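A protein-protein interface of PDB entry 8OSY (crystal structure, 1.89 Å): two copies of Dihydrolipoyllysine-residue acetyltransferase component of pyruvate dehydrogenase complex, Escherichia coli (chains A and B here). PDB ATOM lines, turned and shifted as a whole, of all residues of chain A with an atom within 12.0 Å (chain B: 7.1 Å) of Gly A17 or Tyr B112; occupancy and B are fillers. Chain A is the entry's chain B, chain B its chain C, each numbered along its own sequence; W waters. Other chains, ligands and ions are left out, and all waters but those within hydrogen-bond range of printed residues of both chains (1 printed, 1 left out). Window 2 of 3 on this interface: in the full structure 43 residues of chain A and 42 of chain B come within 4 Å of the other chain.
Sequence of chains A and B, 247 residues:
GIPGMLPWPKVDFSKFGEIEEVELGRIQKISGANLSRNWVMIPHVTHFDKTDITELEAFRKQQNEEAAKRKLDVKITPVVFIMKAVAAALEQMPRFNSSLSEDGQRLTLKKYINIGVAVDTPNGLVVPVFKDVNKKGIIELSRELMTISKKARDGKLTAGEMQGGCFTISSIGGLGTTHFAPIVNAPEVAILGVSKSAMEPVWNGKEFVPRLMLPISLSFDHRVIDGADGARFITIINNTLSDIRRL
OH of Tyr B112 lies within hydrogen-bond range of O of Phe A13.
O of Glu A18 lies within hydrogen-bond range of N of Lys B111, 2.9 Å away.
The backbone carbonyl oxygen of Glu A20 sits at hydrogen-bond distance from the backbone NH of Leu B109, 2.8 Å away.
OE1 of Glu A20 is in salt-bridge range of NZ of Lys B111, at 3.1 Å.
O of Asn B97 is in hydrogen-bond range of N of Lys B110 (3.0 Å).
ND2 of Asn B97 is in hydrogen-bond range of O of Tyr B112, 2.8 Å away.
The backbone carbonyl oxygen (O) of Ser B99 lies within hydrogen-bond range of the backbone NH (N) of Thr B108.
The side-chain hydroxyl (OG) of Ser B99 sits at hydrogen-bond distance from the side-chain amino group (NZ) of Lys B110 (2.8 Å).
SG of Cys B166 lies close to O of Tyr B112.
ND2 of Asn B114 sits at hydrogen-bond distance from O of Gly B164, at 3.0 Å.
Among the printed residues, pairs that only touch across the chains: Phe A13 with Ser B99 (3.4 Å), Phe A13 with Lys B110 (3.5 Å), Phe A16 with Tyr B112 (3.6 Å), Phe A16 with Gly B164 (3.4 Å), Gly A17 with Tyr B112 (3.5 Å), Glu A18 with Lys B110 (3.9 Å), Glu A18 with Tyr B112 (3.8 Å), Ile A19 with Thr B108 (3.9 Å), Ile A19 with Leu B109 (3.3 Å), Ile A19 with Tyr B112 (3.9 Å), Glu A20 with Thr B108 (3.7 Å) and Glu A21 with Thr B108 (3.9 Å).
Of the printed residues of chain B, Phe A16 touches Tyr B112 (3.6 Å) and Gly B164 (3.4 Å).
Gly A17 touches one residue of chain B.
Printed residues of chain B within 4 Å of Glu A20: Thr B108, Leu B109 and Lys B111.
Asn B97 touches none of the printed residues of chain A.
Printed residues of chain A within 4 Å of Thr B108: Ile A19, Glu A20 and Glu A21.
Printed residues of chain A within 4 Å of Leu B109: Ile A19 and Glu A20.
Of chain A, only Phe A13 (3.5 Å) and Glu A18 (3.9 Å) come within 4 Å of Lys B110.
Tyr B112 touches five residues of chain A.
No residue of chain A comes within 4 Å of Asn B114.
Of chain A, only Phe A16 comes within 4 Å of Gly B164.
The nearest residue of chain B that does not touch Gly A17 is Lys B111 (5.8 Å).
Printed residues of chain B that touch a printed residue of chain A: Ser B99, Thr B108, Leu B109, Lys B110, Lys B111, Tyr B112 and Gly B164.
Among the printed residues, 16 pairs touch across the chains.
Among the printed residues, Asp or Glu carboxylates within 4 Å of a Lys or Arg side-chain nitrogen of the other chain: Glu A20 with Lys B111.
No position is printed for both chains.
Of the 16 pairs that touch across the chains among the printed residues, none has its exchanged pair printed and touching as well.
Water W1 lies within hydrogen-bond range of the side-chain hydroxyl of Thr B108 and the side-chain carboxylate of Glu A21.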
ATOM      1  N   PRO A   9       0.820 -14.587   7.541  1.00  0.00           N
ATOM      2  CA  PRO A   9       1.399 -14.244   8.845  1.00  0.00           C
ATOM      3  C   PRO A   9       1.514 -12.737   9.016  1.00  0.00           C
ATOM      4  O   PRO A   9       1.831 -12.009   8.072  1.00  0.00           O
ATOM      5  CB  PRO A   9       2.778 -14.910   8.815  1.00  0.00           C
ATOM      6  CG  PRO A   9       2.687 -15.976   7.730  1.00  0.00           C
ATOM      7  CD  PRO A   9       1.727 -15.418   6.722  1.00  0.00           C
ATOM      8  N   LYS A  10       1.242 -12.277  10.235  1.00  0.00           N
ATOM      9  CA  LYS A  10       1.436 -10.889  10.636  1.00  0.00           C
ATOM     10  C   LYS A  10       2.567 -10.837  11.653  1.00  0.00           C
ATOM     11  O   LYS A  10       2.426 -11.356  12.768  1.00  0.00           O
ATOM     12  CB  LYS A  10       0.160 -10.293  11.239  1.00  0.00           C
ATOM     13  CG  LYS A  10      -0.779  -9.654  10.217  1.00  0.00           C
ATOM     14  CD  LYS A  10      -0.059  -8.668   9.291  1.00  0.00           C
ATOM     15  CE  LYS A  10       0.661  -7.560  10.055  1.00  0.00           C
ATOM     16  NZ  LYS A  10       0.988  -6.405   9.173  1.00  0.00           N
ATOM     17  N   VAL A  11       3.677 -10.208  11.278  1.00  0.00           N
ATOM     18  CA  VAL A  11       4.876 -10.195  12.105  1.00  0.00           C
ATOM     19  C   VAL A  11       5.409  -8.768  12.156  1.00  0.00           C
ATOM     20  O   VAL A  11       5.536  -8.112  11.116  1.00  0.00           O
ATOM     21  CB  VAL A  11       5.954 -11.153  11.553  1.00  0.00           C
ATOM     22  CG1 VAL A  11       7.308 -10.875  12.189  1.00  0.00           C
ATOM     23  CG2 VAL A  11       5.540 -12.612  11.740  1.00  0.00           C
ATOM     24  N   ASP A  12       5.727  -8.294  13.359  1.00  0.00           N
ATOM     25  CA  ASP A  12       6.383  -7.001  13.560  1.00  0.00           C
ATOM     26  C   ASP A  12       7.878  -7.207  13.369  1.00  0.00           C
ATOM     27  O   ASP A  12       8.624  -7.440  14.320  1.00  0.00           O
ATOM     28  CB  ASP A  12       6.064  -6.440  14.944  1.00  0.00           C
ATOM     29  CG  ASP A  12       6.724  -5.089  15.199  1.00  0.00           C
ATOM     30  OD1 ASP A  12       7.302  -4.508  14.258  1.00  0.00           O
ATOM     31  OD2 ASP A  12       6.658  -4.605  16.345  1.00  0.00           O
ATOM     32  N   PHE A  13       8.321  -7.101  12.113  1.00  0.00           N
ATOM     33  CA  PHE A  13       9.716  -7.373  11.784  1.00  0.00           C
ATOM     34  C   PHE A  13      10.667  -6.403  12.465  1.00  0.00           C
ATOM     35  O   PHE A  13      11.835  -6.742  12.684  1.00  0.00           O
ATOM     36  CB  PHE A  13       9.919  -7.323  10.271  1.00  0.00           C
ATOM     37  CG  PHE A  13       9.141  -8.363   9.521  1.00  0.00           C
ATOM     38  CD1 PHE A  13       9.405  -9.715   9.710  1.00  0.00           C
ATOM     39  CD2 PHE A  13       8.153  -7.994   8.625  1.00  0.00           C
ATOM     40  CE1 PHE A  13       8.693 -10.686   9.023  1.00  0.00           C
ATOM     41  CE2 PHE A  13       7.435  -8.952   7.929  1.00  0.00           C
ATOM     42  CZ  PHE A  13       7.704 -10.308   8.132  1.00  0.00           C
ATOM     43  N   SER A  14      10.193  -5.194  12.801  1.00  0.00           N
ATOM     44  CA  SER A  14      11.072  -4.199  13.405  1.00  0.00           C
ATOM     45  C   SER A  14      11.602  -4.639  14.762  1.00  0.00           C
ATOM     46  O   SER A  14      12.613  -4.101  15.222  1.00  0.00           O
ATOM     47  CB  SER A  14      10.357  -2.846  13.543  1.00  0.00           C
ATOM     48  OG  SER A  14       9.356  -2.869  14.548  1.00  0.00           O
ATOM     49  N   LYS A  15      10.970  -5.618  15.410  1.00  0.00           N
ATOM     50  CA  LYS A  15      11.458  -6.024  16.722  1.00  0.00           C
ATOM     51  C   LYS A  15      12.715  -6.890  16.652  1.00  0.00           C
ATOM     52  O   LYS A  15      13.356  -7.108  17.686  1.00  0.00           O
ATOM     53  CB  LYS A  15      10.349  -6.743  17.498  1.00  0.00           C
ATOM     54  CG  LYS A  15      10.418  -8.259  17.478  1.00  0.00           C
ATOM     55  CD  LYS A  15       9.615  -8.805  18.649  1.00  0.00           C
ATOM     56  CE  LYS A  15       9.821 -10.298  18.833  1.00  0.00           C
ATOM     57  NZ  LYS A  15       9.136 -10.768  20.078  1.00  0.00           N
ATOM     58  N   PHE A  16      13.096  -7.370  15.469  1.00  0.00           N
ATOM     59  CA  PHE A  16      14.323  -8.136  15.294  1.00  0.00           C
ATOM     60  C   PHE A  16      15.485  -7.301  14.765  1.00  0.00           C
ATOM     61  O   PHE A  16      16.635  -7.746  14.851  1.00  0.00           O
ATOM     62  CB  PHE A  16      14.072  -9.325  14.349  1.00  0.00           C
ATOM     63  CG  PHE A  16      12.941 -10.200  14.788  1.00  0.00           C
ATOM     64  CD1 PHE A  16      13.080 -11.022  15.896  1.00  0.00           C
ATOM     65  CD2 PHE A  16      11.727 -10.178  14.121  1.00  0.00           C
ATOM     66  CE1 PHE A  16      12.035 -11.824  16.325  1.00  0.00           C
ATOM     67  CE2 PHE A  16      10.674 -10.978  14.547  1.00  0.00           C
ATOM     68  CZ  PHE A  16      10.832 -11.802  15.646  1.00  0.00           C
ATOM     69  N   GLY A  17      15.221  -6.119  14.227  1.00  0.00           N
ATOM     70  CA  GLY A  17      16.279  -5.267  13.728  1.00  0.00           C
ATOM     71  C   GLY A  17      15.715  -4.210  12.797  1.00  0.00           C
ATOM     72  O   GLY A  17      14.506  -3.979  12.740  1.00  0.00           O
ATOM     73  N   GLU A  18      16.623  -3.584  12.058  1.00  0.00           N
ATOM     74  CA  GLU A  18      16.243  -2.515  11.149  1.00  0.00           C
ATOM     75  C   GLU A  18      15.557  -3.079   9.912  1.00  0.00           C
ATOM     76  O   GLU A  18      15.954  -4.125   9.384  1.00  0.00           O
ATOM     77  CB  GLU A  18      17.478  -1.698  10.763  1.00  0.00           C
ATOM     78  CG  GLU A  18      17.239  -0.605   9.751  1.00  0.00           C
ATOM     79  CD  GLU A  18      18.518   0.144   9.397  1.00  0.00           C
ATOM     80  OE1 GLU A  18      19.620  -0.367   9.694  1.00  0.00           O
ATOM     81  OE2 GLU A  18      18.420   1.251   8.827  1.00  0.00           O
ATOM     82  N   ILE A  19      14.508  -2.389   9.456  1.00  0.00           N
ATOM     83  CA  ILE A  19      13.785  -2.781   8.255  1.00  0.00           C
ATOM     84  C   ILE A  19      13.549  -1.554   7.385  1.00  0.00           C
ATOM     85  O   ILE A  19      13.635  -0.413   7.841  1.00  0.00           O
ATOM     86  CB  ILE A  19      12.439  -3.461   8.573  1.00  0.00           C
ATOM     87  CG1 ILE A  19      11.556  -2.533   9.414  1.00  0.00           C
ATOM     88  CG2 ILE A  19      12.672  -4.796   9.287  1.00  0.00           C
ATOM     89  CD1 ILE A  19      10.117  -2.996   9.506  1.00  0.00           C
ATOM     90  N   GLU A  20      13.230  -1.812   6.117  1.00  0.00           N
ATOM     91  CA  GLU A  20      12.858  -0.771   5.168  1.00  0.00           C
ATOM     92  C   GLU A  20      11.774  -1.324   4.260  1.00  0.00           C
ATOM     93  O   GLU A  20      12.005  -2.292   3.527  1.00  0.00           O
ATOM     94  CB  GLU A  20      14.061  -0.300   4.347  1.00  0.00           C
ATOM     95  CG  GLU A  20      13.703   0.709   3.271  1.00  0.00           C
ATOM     96  CD  GLU A  20      14.768   0.820   2.200  1.00  0.00           C
ATOM     97  OE1 GLU A  20      15.812   0.142   2.319  1.00  0.00           O
ATOM     98  OE2 GLU A  20      14.556   1.575   1.229  1.00  0.00           O
ATOM     99  N   GLU A  21      10.596  -0.722   4.318  1.00  0.00           N
ATOM    100  CA  GLU A  21       9.448  -1.188   3.555  1.00  0.00           C
ATOM    101  C   GLU A  21       9.386  -0.424   2.236  1.00  0.00           C
ATOM    102  O   GLU A  21       9.187   0.791   2.235  1.00  0.00           O
ATOM    103  CB  GLU A  21       8.180  -0.977   4.382  1.00  0.00           C
ATOM    104  CG  GLU A  21       6.953  -1.754   3.944  1.00  0.00           C
ATOM    105  CD  GLU A  21       5.766  -1.474   4.857  1.00  0.00           C
ATOM    106  OE1 GLU A  21       5.877  -1.742   6.075  1.00  0.00           O
ATOM    107  OE2 GLU A  21       4.737  -0.953   4.367  1.00  0.00           O
ATOM    108  N   LEU B  90      22.727 -13.530   1.332  1.00  0.00           N
ATOM    109  CA  LEU B  90      21.704 -12.586   1.761  1.00  0.00           C
ATOM    110  C   LEU B  90      22.264 -11.173   1.868  1.00  0.00           C
ATOM    111  O   LEU B  90      21.547 -10.202   1.597  1.00  0.00           O
ATOM    112  CB  LEU B  90      21.109 -13.040   3.098  1.00  0.00           C
ATOM    113  CG  LEU B  90      20.329 -14.368   3.051  1.00  0.00           C
ATOM    114  CD1 LEU B  90      19.930 -14.837   4.450  1.00  0.00           C
ATOM    115  CD2 LEU B  90      19.101 -14.260   2.167  1.00  0.00           C
ATOM    116  N   ASN B  97      16.508 -11.307   1.410  1.00  0.00           N
ATOM    117  CA  ASN B  97      16.334 -11.138   2.851  1.00  0.00           C
ATOM    118  C   ASN B  97      15.157 -10.192   3.080  1.00  0.00           C
ATOM    119  O   ASN B  97      15.321  -9.021   3.417  1.00  0.00           O
ATOM    120  CB  ASN B  97      17.613 -10.591   3.478  1.00  0.00           C
ATOM    121  CG  ASN B  97      17.523 -10.527   4.976  1.00  0.00           C
ATOM    122  OD1 ASN B  97      16.562 -11.039   5.558  1.00  0.00           O
ATOM    123  ND2 ASN B  97      18.478  -9.850   5.612  1.00  0.00           N
ATOM    124  N   SER B  99      10.416  -9.855   3.168  1.00  0.00           N
ATOM    125  CA  SER B  99       9.091 -10.440   3.306  1.00  0.00           C
ATOM    126  C   SER B  99       8.090  -9.585   2.554  1.00  0.00           C
ATOM    127  O   SER B  99       8.076  -8.355   2.696  1.00  0.00           O
ATOM    128  CB  SER B  99       8.676 -10.567   4.772  1.00  0.00           C
ATOM    129  OG  SER B  99       9.544 -11.436   5.467  1.00  0.00           O
ATOM    130  N   THR B 108       9.205  -5.759   2.530  1.00  0.00           N
ATOM    131  CA  THR B 108       9.988  -5.365   3.694  1.00  0.00           C
ATOM    132  C   THR B 108      11.399  -5.921   3.550  1.00  0.00           C
ATOM    133  O   THR B 108      11.609  -7.134   3.652  1.00  0.00           O
ATOM    134  CB  THR B 108       9.327  -5.875   4.972  1.00  0.00           C
ATOM    135  OG1 THR B 108       8.021  -5.295   5.090  1.00  0.00           O
ATOM    136  CG2 THR B 108      10.176  -5.529   6.199  1.00  0.00           C
ATOM    137  N   LEU B 109      12.362  -5.036   3.307  1.00  0.00           N
ATOM    138  CA  LEU B 109      13.769  -5.409   3.285  1.00  0.00           C
ATOM    139  C   LEU B 109      14.312  -5.432   4.705  1.00  0.00           C
ATOM    140  O   LEU B 109      14.175  -4.452   5.448  1.00  0.00           O
ATOM    141  CB  LEU B 109      14.572  -4.422   2.430  1.00  0.00           C
ATOM    142  CG  LEU B 109      14.147  -4.304   0.971  1.00  0.00           C
ATOM    143  CD1 LEU B 109      14.894  -3.170   0.278  1.00  0.00           C
ATOM    144  CD2 LEU B 109      14.395  -5.630   0.256  1.00  0.00           C
ATOM    145  N   LYS B 110      14.933  -6.546   5.076  1.00  0.00           N
ATOM    146  CA  LYS B 110      15.488  -6.742   6.407  1.00  0.00           C
ATOM    147  C   LYS B 110      16.983  -6.447   6.407  1.00  0.00           C
ATOM    148  O   LYS B 110      17.714  -6.884   5.514  1.00  0.00           O
ATOM    149  CB  LYS B 110      15.231  -8.179   6.885  1.00  0.00           C
ATOM    150  CG  LYS B 110      13.751  -8.517   6.979  1.00  0.00           C
ATOM    151  CD  LYS B 110      13.484 -10.015   7.156  1.00  0.00           C
ATOM    152  CE  LYS B 110      11.988 -10.263   7.166  1.00  0.00           C
ATOM    153  NZ  LYS B 110      11.630 -11.685   7.389  1.00  0.00           N
ATOM    154  N   LYS B 111      17.436  -5.712   7.417  1.00  0.00           N
ATOM    155  CA  LYS B 111      18.849  -5.410   7.582  1.00  0.00           C
ATOM    156  C   LYS B 111      19.532  -6.335   8.578  1.00  0.00           C
ATOM    157  O   LYS B 111      20.737  -6.196   8.811  1.00  0.00           O
ATOM    158  CB  LYS B 111      19.026  -3.954   8.023  1.00  0.00           C
ATOM    159  CG  LYS B 111      18.163  -2.961   7.255  1.00  0.00           C
ATOM    160  CD  LYS B 111      18.430  -2.975   5.758  1.00  0.00           C
ATOM    161  CE  LYS B 111      17.467  -2.034   5.041  1.00  0.00           C
ATOM    162  NZ  LYS B 111      17.745  -1.892   3.585  1.00  0.00           N
ATOM    163  N   TYR B 112      18.786  -7.248   9.191  1.00  0.00           N
ATOM    164  CA  TYR B 112      19.318  -8.282  10.062  1.00  0.00           C
ATOM    165  C   TYR B 112      19.247  -9.609   9.322  1.00  0.00           C
ATOM    166  O   TYR B 112      18.456  -9.767   8.396  1.00  0.00           O
ATOM    167  CB  TYR B 112      18.522  -8.376  11.364  1.00  0.00           C
ATOM    168  CG  TYR B 112      17.036  -8.594  11.160  1.00  0.00           C
ATOM    169  CD1 TYR B 112      16.169  -7.516  11.007  1.00  0.00           C
ATOM    170  CD2 TYR B 112      16.505  -9.879  11.104  1.00  0.00           C
ATOM    171  CE1 TYR B 112      14.811  -7.715  10.824  1.00  0.00           C
ATOM    172  CE2 TYR B 112      15.155 -10.090  10.919  1.00  0.00           C
ATOM    173  CZ  TYR B 112      14.312  -9.011  10.778  1.00  0.00           C
ATOM    174  OH  TYR B 112      12.968  -9.231  10.596  1.00  0.00           O
ATOM    175  N   ILE B 113      20.071 -10.567   9.738  1.00  0.00           N
ATOM    176  CA  ILE B 113      20.187 -11.849   9.038  1.00  0.00           C
ATOM    177  C   ILE B 113      20.052 -12.966  10.066  1.00  0.00           C
ATOM    178  O   ILE B 113      21.004 -13.269  10.795  1.00  0.00           O
ATOM    179  CB  ILE B 113      21.496 -11.970   8.253  1.00  0.00           C
ATOM    180  CG1 ILE B 113      21.540 -10.910   7.155  1.00  0.00           C
ATOM    181  CG2 ILE B 113      21.621 -13.363   7.621  1.00  0.00           C
ATOM    182  CD1 ILE B 113      22.724 -11.039   6.245  1.00  0.00           C
ATOM    183  N   ASN B 114      18.861 -13.564  10.137  1.00  0.00           N
ATOM    184  CA  ASN B 114      18.585 -14.728  10.969  1.00  0.00           C
ATOM    185  C   ASN B 114      18.156 -15.878  10.066  1.00  0.00           C
ATOM    186  O   ASN B 114      17.351 -15.688   9.148  1.00  0.00           O
ATOM    187  CB  ASN B 114      17.478 -14.455  11.998  1.00  0.00           C
ATOM    188  CG  ASN B 114      17.720 -13.195  12.842  1.00  0.00           C
ATOM    189  OD1 ASN B 114      18.854 -12.840  13.181  1.00  0.00           O
ATOM    190  ND2 ASN B 114      16.629 -12.536  13.208  1.00  0.00           N
ATOM    191  N   LYS B 131      20.333 -16.368  15.168  1.00  0.00           N
ATOM    192  CA  LYS B 131      20.365 -14.938  14.905  1.00  0.00           C
ATOM    193  C   LYS B 131      21.764 -14.456  14.547  1.00  0.00           C
ATOM    194  O   LYS B 131      22.770 -14.985  15.028  1.00  0.00           O
ATOM    195  CB  LYS B 131      19.830 -14.155  16.105  1.00  0.00           C
ATOM    196  CG  LYS B 131      18.570 -14.764  16.683  1.00  0.00           C
ATOM    197  CD  LYS B 131      17.369 -13.849  16.481  1.00  0.00           C
ATOM    198  CE  LYS B 131      16.163 -14.339  17.276  1.00  0.00           C
ATOM    199  NZ  LYS B 131      15.519 -15.510  16.593  1.00  0.00           N
ATOM    200  N   ASP B 132      21.807 -13.437  13.684  1.00  0.00           N
ATOM    201  CA  ASP B 132      23.043 -12.741  13.321  1.00  0.00           C
ATOM    202  C   ASP B 132      24.113 -13.721  12.840  1.00  0.00           C
ATOM    203  O   ASP B 132      25.256 -13.722  13.304  1.00  0.00           O
ATOM    204  CB  ASP B 132      23.545 -11.882  14.484  1.00  0.00           C
ATOM    205  CG  ASP B 132      22.553 -10.800  14.873  1.00  0.00           C
ATOM    206  OD1 ASP B 132      22.017 -10.137  13.964  1.00  0.00           O
ATOM    207  OD2 ASP B 132      22.323 -10.592  16.085  1.00  0.00           O
ATOM    208  N   ASN B 134      25.540 -13.768   9.974  1.00  0.00           N
ATOM    209  CA  ASN B 134      26.584 -13.044   9.262  1.00  0.00           C
ATOM    210  C   ASN B 134      27.633 -12.452  10.197  1.00  0.00           C
ATOM    211  O   ASN B 134      28.725 -12.106   9.737  1.00  0.00           O
ATOM    212  CB  ASN B 134      25.955 -11.933   8.423  1.00  0.00           C
ATOM    213  CG  ASN B 134      25.192 -10.926   9.267  1.00  0.00           C
ATOM    214  OD1 ASN B 134      24.522 -11.284  10.240  1.00  0.00           O
ATOM    215  ND2 ASN B 134      25.282  -9.659   8.891  1.00  0.00           N
ATOM    216  N   LYS B 135      27.336 -12.328  11.489  1.00  0.00           N
ATOM    217  CA  LYS B 135      28.270 -11.759  12.449  1.00  0.00           C
ATOM    218  C   LYS B 135      28.893 -12.802  13.365  1.00  0.00           C
ATOM    219  O   LYS B 135      29.686 -12.445  14.243  1.00  0.00           O
ATOM    220  CB  LYS B 135      27.568 -10.686  13.290  1.00  0.00           C
ATOM    221  CG  LYS B 135      26.975  -9.557  12.465  1.00  0.00           C
ATOM    222  CD  LYS B 135      26.400  -8.464  13.347  1.00  0.00           C
ATOM    223  CE  LYS B 135      25.854  -7.321  12.513  1.00  0.00           C
ATOM    224  NZ  LYS B 135      26.903  -6.685  11.663  1.00  0.00           N
ATOM    225  N   GLY B 164      11.788 -14.705  14.183  1.00  0.00           N
ATOM    226  CA  GLY B 164      12.745 -13.826  13.528  1.00  0.00           C
ATOM    227  C   GLY B 164      13.396 -14.337  12.260  1.00  0.00           C
ATOM    228  O   GLY B 164      14.293 -13.660  11.734  1.00  0.00           O
ATOM    229  N   GLY B 165      12.953 -15.473  11.726  1.00  0.00           N
ATOM    230  CA  GLY B 165      13.645 -16.079  10.597  1.00  0.00           C
ATOM    231  C   GLY B 165      13.591 -15.219   9.341  1.00  0.00           C
ATOM    232  O   GLY B 165      12.585 -14.572   9.041  1.00  0.00           O
ATOM    233  N   CYS B 166      14.709 -15.204   8.607  1.00  0.00           N
ATOM    234  CA  CYS B 166      14.793 -14.519   7.320  1.00  0.00           C
ATOM    235  C   CYS B 166      14.854 -15.467   6.137  1.00  0.00           C
ATOM    236  O   CYS B 166      14.637 -15.033   5.001  1.00  0.00           O
ATOM    237  CB  CYS B 166      16.037 -13.624   7.252  1.00  0.00           C
ATOM    238  SG  CYS B 166      16.216 -12.436   8.573  1.00  0.00           S
HETATM  239  O   HOH W   1       6.927  -4.288   7.399  1.00  0.00           O
